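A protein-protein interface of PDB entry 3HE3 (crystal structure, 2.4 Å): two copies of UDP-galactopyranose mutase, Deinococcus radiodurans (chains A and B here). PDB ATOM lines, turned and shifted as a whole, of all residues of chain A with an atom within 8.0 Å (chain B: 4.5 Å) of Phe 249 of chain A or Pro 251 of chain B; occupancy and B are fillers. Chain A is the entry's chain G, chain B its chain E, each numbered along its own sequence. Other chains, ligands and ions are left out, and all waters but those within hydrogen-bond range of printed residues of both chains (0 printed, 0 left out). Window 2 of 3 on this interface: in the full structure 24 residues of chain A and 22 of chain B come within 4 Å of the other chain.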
ATOM      1  N   LYS A  28      40.064 -22.106  20.050  1.00  0.00           N
ATOM      2  CA  LYS A  28      39.762 -21.323  21.238  1.00  0.00           C
ATOM      3  C   LYS A  28      38.432 -21.665  21.906  1.00  0.00           C
ATOM      4  O   LYS A  28      37.784 -22.646  21.569  1.00  0.00           O
ATOM      5  CB  LYS A  28      39.794 -19.838  20.907  1.00  0.00           C
ATOM      6  CG  LYS A  28      38.791 -19.406  19.862  1.00  0.00           C
ATOM      7  CD  LYS A  28      38.883 -17.924  19.589  1.00  0.00           C
ATOM      8  CE  LYS A  28      37.571 -17.217  19.872  1.00  0.00           C
ATOM      9  NZ  LYS A  28      37.360 -16.013  19.031  1.00  0.00           N
ATOM     10  N   MET A 238      26.985 -21.400  33.825  1.00  0.00           N
ATOM     11  CA  MET A 238      26.071 -20.400  33.308  1.00  0.00           C
ATOM     12  C   MET A 238      24.632 -20.817  33.587  1.00  0.00           C
ATOM     13  O   MET A 238      24.164 -21.844  33.094  1.00  0.00           O
ATOM     14  CB  MET A 238      26.301 -20.210  31.816  1.00  0.00           C
ATOM     15  CG  MET A 238      26.038 -18.807  31.330  1.00  0.00           C
ATOM     16  SD  MET A 238      26.518 -18.620  29.607  1.00  0.00           S
ATOM     17  CE  MET A 238      25.752 -17.042  29.236  1.00  0.00           C
ATOM     18  N   THR A 241      20.171 -19.694  31.498  1.00  0.00           N
ATOM     19  CA  THR A 241      20.566 -19.596  30.100  1.00  0.00           C
ATOM     20  C   THR A 241      20.208 -20.838  29.291  1.00  0.00           C
ATOM     21  O   THR A 241      20.648 -21.945  29.603  1.00  0.00           O
ATOM     22  CB  THR A 241      22.082 -19.347  29.963  1.00  0.00           C
ATOM     23  OG1 THR A 241      22.450 -18.176  30.702  1.00  0.00           O
ATOM     24  CG2 THR A 241      22.461 -19.164  28.500  1.00  0.00           C
ATOM     25  N   TYR A 243      20.852 -22.903  26.008  1.00  0.00           N
ATOM     26  CA  TYR A 243      22.044 -23.021  25.171  1.00  0.00           C
ATOM     27  C   TYR A 243      21.881 -22.275  23.851  1.00  0.00           C
ATOM     28  O   TYR A 243      22.839 -21.704  23.323  1.00  0.00           O
ATOM     29  CB  TYR A 243      22.408 -24.491  24.930  1.00  0.00           C
ATOM     30  CG  TYR A 243      21.557 -25.197  23.901  1.00  0.00           C
ATOM     31  CD1 TYR A 243      22.015 -25.385  22.602  1.00  0.00           C
ATOM     32  CD2 TYR A 243      20.304 -25.689  24.229  1.00  0.00           C
ATOM     33  CE1 TYR A 243      21.243 -26.037  21.658  1.00  0.00           C
ATOM     34  CE2 TYR A 243      19.523 -26.344  23.291  1.00  0.00           C
ATOM     35  CZ  TYR A 243      19.997 -26.512  22.008  1.00  0.00           C
ATOM     36  OH  TYR A 243      19.220 -27.161  21.077  1.00  0.00           O
ATOM     37  N   ARG A 244      20.661 -22.264  23.329  1.00  0.00           N
ATOM     38  CA  ARG A 244      20.395 -21.602  22.059  1.00  0.00           C
ATOM     39  C   ARG A 244      20.676 -20.099  22.096  1.00  0.00           C
ATOM     40  O   ARG A 244      20.902 -19.485  21.056  1.00  0.00           O
ATOM     41  CB  ARG A 244      18.960 -21.867  21.604  1.00  0.00           C
ATOM     42  CG  ARG A 244      18.698 -23.317  21.213  1.00  0.00           C
ATOM     43  CD  ARG A 244      17.238 -23.536  20.856  1.00  0.00           C
ATOM     44  NE  ARG A 244      16.368 -23.426  22.023  1.00  0.00           N
ATOM     45  CZ  ARG A 244      15.889 -24.466  22.698  1.00  0.00           C
ATOM     46  NH1 ARG A 244      16.193 -25.700  22.316  1.00  0.00           N
ATOM     47  NH2 ARG A 244      15.102 -24.277  23.749  1.00  0.00           N
ATOM     48  N   GLU A 245      20.679 -19.509  23.285  1.00  0.00           N
ATOM     49  CA  GLU A 245      20.928 -18.072  23.406  1.00  0.00           C
ATOM     50  C   GLU A 245      22.412 -17.720  23.321  1.00  0.00           C
ATOM     51  O   GLU A 245      22.764 -16.549  23.186  1.00  0.00           O
ATOM     52  CB  GLU A 245      20.354 -17.515  24.713  1.00  0.00           C
ATOM     53  CG  GLU A 245      18.941 -17.963  25.042  1.00  0.00           C
ATOM     54  CD  GLU A 245      18.329 -17.155  26.175  1.00  0.00           C
ATOM     55  OE1 GLU A 245      18.134 -17.709  27.280  1.00  0.00           O
ATOM     56  OE2 GLU A 245      18.055 -15.955  25.960  1.00  0.00           O
ATOM     57  N   ILE A 246      23.281 -18.727  23.406  1.00  0.00           N
ATOM     58  CA  ILE A 246      24.724 -18.486  23.400  1.00  0.00           C
ATOM     59  C   ILE A 246      25.478 -19.347  22.391  1.00  0.00           C
ATOM     60  O   ILE A 246      26.665 -19.132  22.148  1.00  0.00           O
ATOM     61  CB  ILE A 246      25.351 -18.741  24.782  1.00  0.00           C
ATOM     62  CG1 ILE A 246      25.166 -20.207  25.182  1.00  0.00           C
ATOM     63  CG2 ILE A 246      24.760 -17.800  25.819  1.00  0.00           C
ATOM     64  CD1 ILE A 246      26.233 -20.721  26.120  1.00  0.00           C
ATOM     65  N   ALA A 247      24.790 -20.325  21.814  1.00  0.00           N
ATOM     66  CA  ALA A 247      25.437 -21.284  20.923  1.00  0.00           C
ATOM     67  C   ALA A 247      26.120 -20.629  19.720  1.00  0.00           C
ATOM     68  O   ALA A 247      27.088 -21.165  19.181  1.00  0.00           O
ATOM     69  CB  ALA A 247      24.438 -22.333  20.460  1.00  0.00           C
ATOM     70  N   ASP A 248      25.622 -19.469  19.307  1.00  0.00           N
ATOM     71  CA  ASP A 248      26.085 -18.841  18.070  1.00  0.00           C
ATOM     72  C   ASP A 248      27.379 -18.043  18.215  1.00  0.00           C
ATOM     73  O   ASP A 248      28.167 -17.970  17.275  1.00  0.00           O
ATOM     74  CB  ASP A 248      24.989 -17.951  17.474  1.00  0.00           C
ATOM     75  CG  ASP A 248      23.656 -18.670  17.351  1.00  0.00           C
ATOM     76  OD1 ASP A 248      23.597 -19.881  17.658  1.00  0.00           O
ATOM     77  OD2 ASP A 248      22.665 -18.022  16.950  1.00  0.00           O
ATOM     78  N   PHE A 249      27.601 -17.440  19.380  1.00  0.00           N
ATOM     79  CA  PHE A 249      28.779 -16.591  19.563  1.00  0.00           C
ATOM     80  C   PHE A 249      29.798 -17.120  20.579  1.00  0.00           C
ATOM     81  O   PHE A 249      30.791 -16.452  20.877  1.00  0.00           O
ATOM     82  CB  PHE A 249      28.367 -15.161  19.918  1.00  0.00           C
ATOM     83  CG  PHE A 249      27.473 -15.067  21.118  1.00  0.00           C
ATOM     84  CD1 PHE A 249      26.098 -15.131  20.978  1.00  0.00           C
ATOM     85  CD2 PHE A 249      28.008 -14.909  22.385  1.00  0.00           C
ATOM     86  CE1 PHE A 249      25.272 -15.044  22.080  1.00  0.00           C
ATOM     87  CE2 PHE A 249      27.186 -14.821  23.493  1.00  0.00           C
ATOM     88  CZ  PHE A 249      25.817 -14.888  23.339  1.00  0.00           C
ATOM     89  N   ILE A 250      29.557 -18.318  21.104  1.00  0.00           N
ATOM     90  CA  ILE A 250      30.502 -18.933  22.033  1.00  0.00           C
ATOM     91  C   ILE A 250      31.182 -20.149  21.417  1.00  0.00           C
ATOM     92  O   ILE A 250      30.514 -21.098  21.002  1.00  0.00           O
ATOM     93  CB  ILE A 250      29.831 -19.337  23.358  1.00  0.00           C
ATOM     94  CG1 ILE A 250      29.494 -18.091  24.180  1.00  0.00           C
ATOM     95  CG2 ILE A 250      30.742 -20.259  24.153  1.00  0.00           C
ATOM     96  CD1 ILE A 250      28.838 -18.391  25.508  1.00  0.00           C
ATOM     97  N   PRO A 251      32.522 -20.121  21.353  1.00  0.00           N
ATOM     98  CA  PRO A 251      33.320 -21.184  20.733  1.00  0.00           C
ATOM     99  C   PRO A 251      33.357 -22.459  21.573  1.00  0.00           C
ATOM    100  O   PRO A 251      33.767 -22.412  22.735  1.00  0.00           O
ATOM    101  CB  PRO A 251      34.731 -20.576  20.665  1.00  0.00           C
ATOM    102  CG  PRO A 251      34.557 -19.114  20.925  1.00  0.00           C
ATOM    103  CD  PRO A 251      33.361 -19.003  21.811  1.00  0.00           C
ATOM    104  N   PHE A 252      32.936 -23.579  20.991  1.00  0.00           N
ATOM    105  CA  PHE A 252      33.105 -24.880  21.630  1.00  0.00           C
ATOM    106  C   PHE A 252      33.308 -25.981  20.594  1.00  0.00           C
ATOM    107  O   PHE A 252      32.709 -25.956  19.518  1.00  0.00           O
ATOM    108  CB  PHE A 252      31.925 -25.204  22.549  1.00  0.00           C
ATOM    109  CG  PHE A 252      30.604 -25.252  21.845  1.00  0.00           C
ATOM    110  CD1 PHE A 252      30.097 -26.454  21.380  1.00  0.00           C
ATOM    111  CD2 PHE A 252      29.867 -24.099  21.652  1.00  0.00           C
ATOM    112  CE1 PHE A 252      28.877 -26.502  20.731  1.00  0.00           C
ATOM    113  CE2 PHE A 252      28.648 -24.140  21.005  1.00  0.00           C
ATOM    114  CZ  PHE A 252      28.152 -25.344  20.545  1.00  0.00           C
ATOM    115  N   LYS B  28      25.624  -9.426  17.642  1.00  0.00           N
ATOM    116  CA  LYS B  28      25.873 -10.618  18.443  1.00  0.00           C
ATOM    117  C   LYS B  28      26.264 -10.251  19.871  1.00  0.00           C
ATOM    118  O   LYS B  28      26.892  -9.216  20.105  1.00  0.00           O
ATOM    119  CB  LYS B  28      26.983 -11.458  17.807  1.00  0.00           C
ATOM    120  CG  LYS B  28      26.883 -11.583  16.296  1.00  0.00           C
ATOM    121  CD  LYS B  28      25.704 -12.450  15.879  1.00  0.00           C
ATOM    122  CE  LYS B  28      25.873 -13.885  16.360  1.00  0.00           C
ATOM    123  NZ  LYS B  28      24.915 -14.815  15.697  1.00  0.00           N
ATOM    124  N   GLY B  29      25.885 -11.099  20.822  1.00  0.00           N
ATOM    125  CA  GLY B  29      26.332 -10.948  22.196  1.00  0.00           C
ATOM    126  C   GLY B  29      25.412 -10.167  23.114  1.00  0.00           C
ATOM    127  O   GLY B  29      24.189 -10.284  23.039  1.00  0.00           O
ATOM    128  N   PHE B  30      26.011  -9.364  23.988  1.00  0.00           N
ATOM    129  CA  PHE B  30      25.266  -8.650  25.016  1.00  0.00           C
ATOM    130  C   PHE B  30      25.487  -7.147  24.944  1.00  0.00           C
ATOM    131  O   PHE B  30      26.546  -6.682  24.528  1.00  0.00           O
ATOM    132  CB  PHE B  30      25.668  -9.147  26.407  1.00  0.00           C
ATOM    133  CG  PHE B  30      25.525 -10.632  26.590  1.00  0.00           C
ATOM    134  CD1 PHE B  30      26.595 -11.480  26.352  1.00  0.00           C
ATOM    135  CD2 PHE B  30      24.322 -11.180  27.005  1.00  0.00           C
ATOM    136  CE1 PHE B  30      26.467 -12.847  26.520  1.00  0.00           C
ATOM    137  CE2 PHE B  30      24.187 -12.547  27.177  1.00  0.00           C
ATOM    138  CZ  PHE B  30      25.261 -13.382  26.935  1.00  0.00           C
ATOM    139  N   PHE B 249      36.387 -13.792  23.849  1.00  0.00           N
ATOM    140  CA  PHE B 249      35.552 -14.416  22.822  1.00  0.00           C
ATOM    141  C   PHE B 249      34.047 -14.191  22.993  1.00  0.00           C
ATOM    142  O   PHE B 249      33.245 -14.758  22.248  1.00  0.00           O
ATOM    143  CB  PHE B 249      35.852 -15.914  22.718  1.00  0.00           C
ATOM    144  CG  PHE B 249      35.936 -16.606  24.043  1.00  0.00           C
ATOM    145  CD1 PHE B 249      37.143 -16.690  24.718  1.00  0.00           C
ATOM    146  CD2 PHE B 249      34.810 -17.171  24.618  1.00  0.00           C
ATOM    147  CE1 PHE B 249      37.227 -17.325  25.940  1.00  0.00           C
ATOM    148  CE2 PHE B 249      34.886 -17.809  25.841  1.00  0.00           C
ATOM    149  CZ  PHE B 249      36.097 -17.884  26.504  1.00  0.00           C
ATOM    150  N   ILE B 250      33.667 -13.367  23.964  1.00  0.00           N
ATOM    151  CA  ILE B 250      32.260 -13.029  24.162  1.00  0.00           C
ATOM    152  C   ILE B 250      31.994 -11.555  23.855  1.00  0.00           C
ATOM    153  O   ILE B 250      32.572 -10.668  24.486  1.00  0.00           O
ATOM    154  CB  ILE B 250      31.780 -13.376  25.589  1.00  0.00           C
ATOM    155  CG1 ILE B 250      31.637 -14.891  25.746  1.00  0.00           C
ATOM    156  CG2 ILE B 250      30.456 -12.697  25.887  1.00  0.00           C
ATOM    157  CD1 ILE B 250      31.080 -15.321  27.089  1.00  0.00           C
ATOM    158  N   PRO B 251      31.121 -11.295  22.869  1.00  0.00           N
ATOM    159  CA  PRO B 251      30.766  -9.958  22.373  1.00  0.00           C
ATOM    160  C   PRO B 251      29.889  -9.156  23.334  1.00  0.00           C
ATOM    161  O   PRO B 251      28.772  -9.572  23.642  1.00  0.00           O
ATOM    162  CB  PRO B 251      29.964 -10.256  21.098  1.00  0.00           C
ATOM    163  CG  PRO B 251      30.260 -11.680  20.760  1.00  0.00           C
ATOM    164  CD  PRO B 251      30.498 -12.358  22.065  1.00  0.00           C
ATOM    165  N   PHE B 252      30.385  -8.007  23.780  1.00  0.00           N
ATOM    166  CA  PHE B 252      29.592  -7.107  24.607  1.00  0.00           C
ATOM    167  C   PHE B 252      29.892  -5.658  24.241  1.00  0.00           C
ATOM    168  O   PHE B 252      31.045  -5.290  24.026  1.00  0.00           O
ATOM    169  CB  PHE B 252      29.884  -7.343  26.085  1.00  0.00           C
ATOM    170  CG  PHE B 252      31.303  -7.066  26.466  1.00  0.00           C
ATOM    171  CD1 PHE B 252      31.652  -5.867  27.061  1.00  0.00           C
ATOM    172  CD2 PHE B 252      32.292  -7.999  26.218  1.00  0.00           C
ATOM    173  CE1 PHE B 252      32.958  -5.610  27.409  1.00  0.00           C
ATOM    174  CE2 PHE B 252      33.601  -7.747  26.565  1.00  0.00           C
ATOM    175  CZ  PHE B 252      33.934  -6.552  27.160  1.00  0.00           C
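Among the printed residues, pairs that only touch across the chains: Lys 28 of chain A with Phe 249 of chain B (3.6 Å), Asp 248 of chain A with Lys 28 of chain B (3.6 Å), Phe 249 of chain A with Phe 30 of chain B (3.7 Å), Phe 249 of chain A with Pro 251 of chain B (3.6 Å) and Pro 251 of chain A with Phe 249 of chain B (3.7 Å).
Pro 251 of chain B touches just one residue of chain A: Phe 249. Printed residues of chain B within 4 Å of Asp 248 of chain A: Lys 28 (3.6 Å). Of the printed residues of chain A, Phe 30 of chain B touches Phe 249 (3.7 Å). Of the printed residues of chain A, Lys 28 of chain B touches Asp 248 (3.6 Å). Of the printed residues of chain A, Phe 249 of chain B touches Lys 28, Phe 249 and Pro 251. Thr 241 of chain A touches none of the printed residues of chain B. Arg 244 of chain A touches none of the printed residues of chain B. The nearest printed residue of chain A that does not touch Lys 28 of chain B is Phe 249 of chain A (4.5 Å).
The backbone carbonyl oxygen (O) of Phe 249 of chain B lies close to the backbone carbonyl oxygen (O) of Phe 249 of chain A (3.3 Å).
The backbone NH (N) of Phe 30 of chain B is in hydrogen-bond range of the backbone carbonyl oxygen (O) of Pro 251 of chain B, 2.8 Å away.
Printed residues of chain A that touch a printed residue of chain B: Lys 28, Asp 248, Phe 249 and Pro 251. Of the 7 printed residues of chain B, 4 touch a printed residue of chain A. Hydrophobic or aromatic side chains of chain B that line the printed part of chain A: Phe 30, Phe 249 and Pro 251. Among the printed residues, 6 pairs touch across the chains. Among the printed residues, no Asp or Glu carboxylate lies within 4 Å of a Lys or Arg side-chain nitrogen of the other chain.
Lys 28 of chain A touches Phe 249 of chain B, but with the chains exchanged Phe 249 of chain A does not touch Lys 28 of chain B (4.5 Å). Phe 249 of chain A touches its own counterpart, Phe 249 of chain B. Phe 249 of chain A touches Pro 251 of chain B, and with the chains exchanged Pro 251 of chain A touches Phe 249 of chain B. Positions printed for both chains: 28, 249, 250, 251 and 252. Of the 6 pairs that touch across the chains among the printed residues, 3 have their exchanged pair printed and touching as well.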
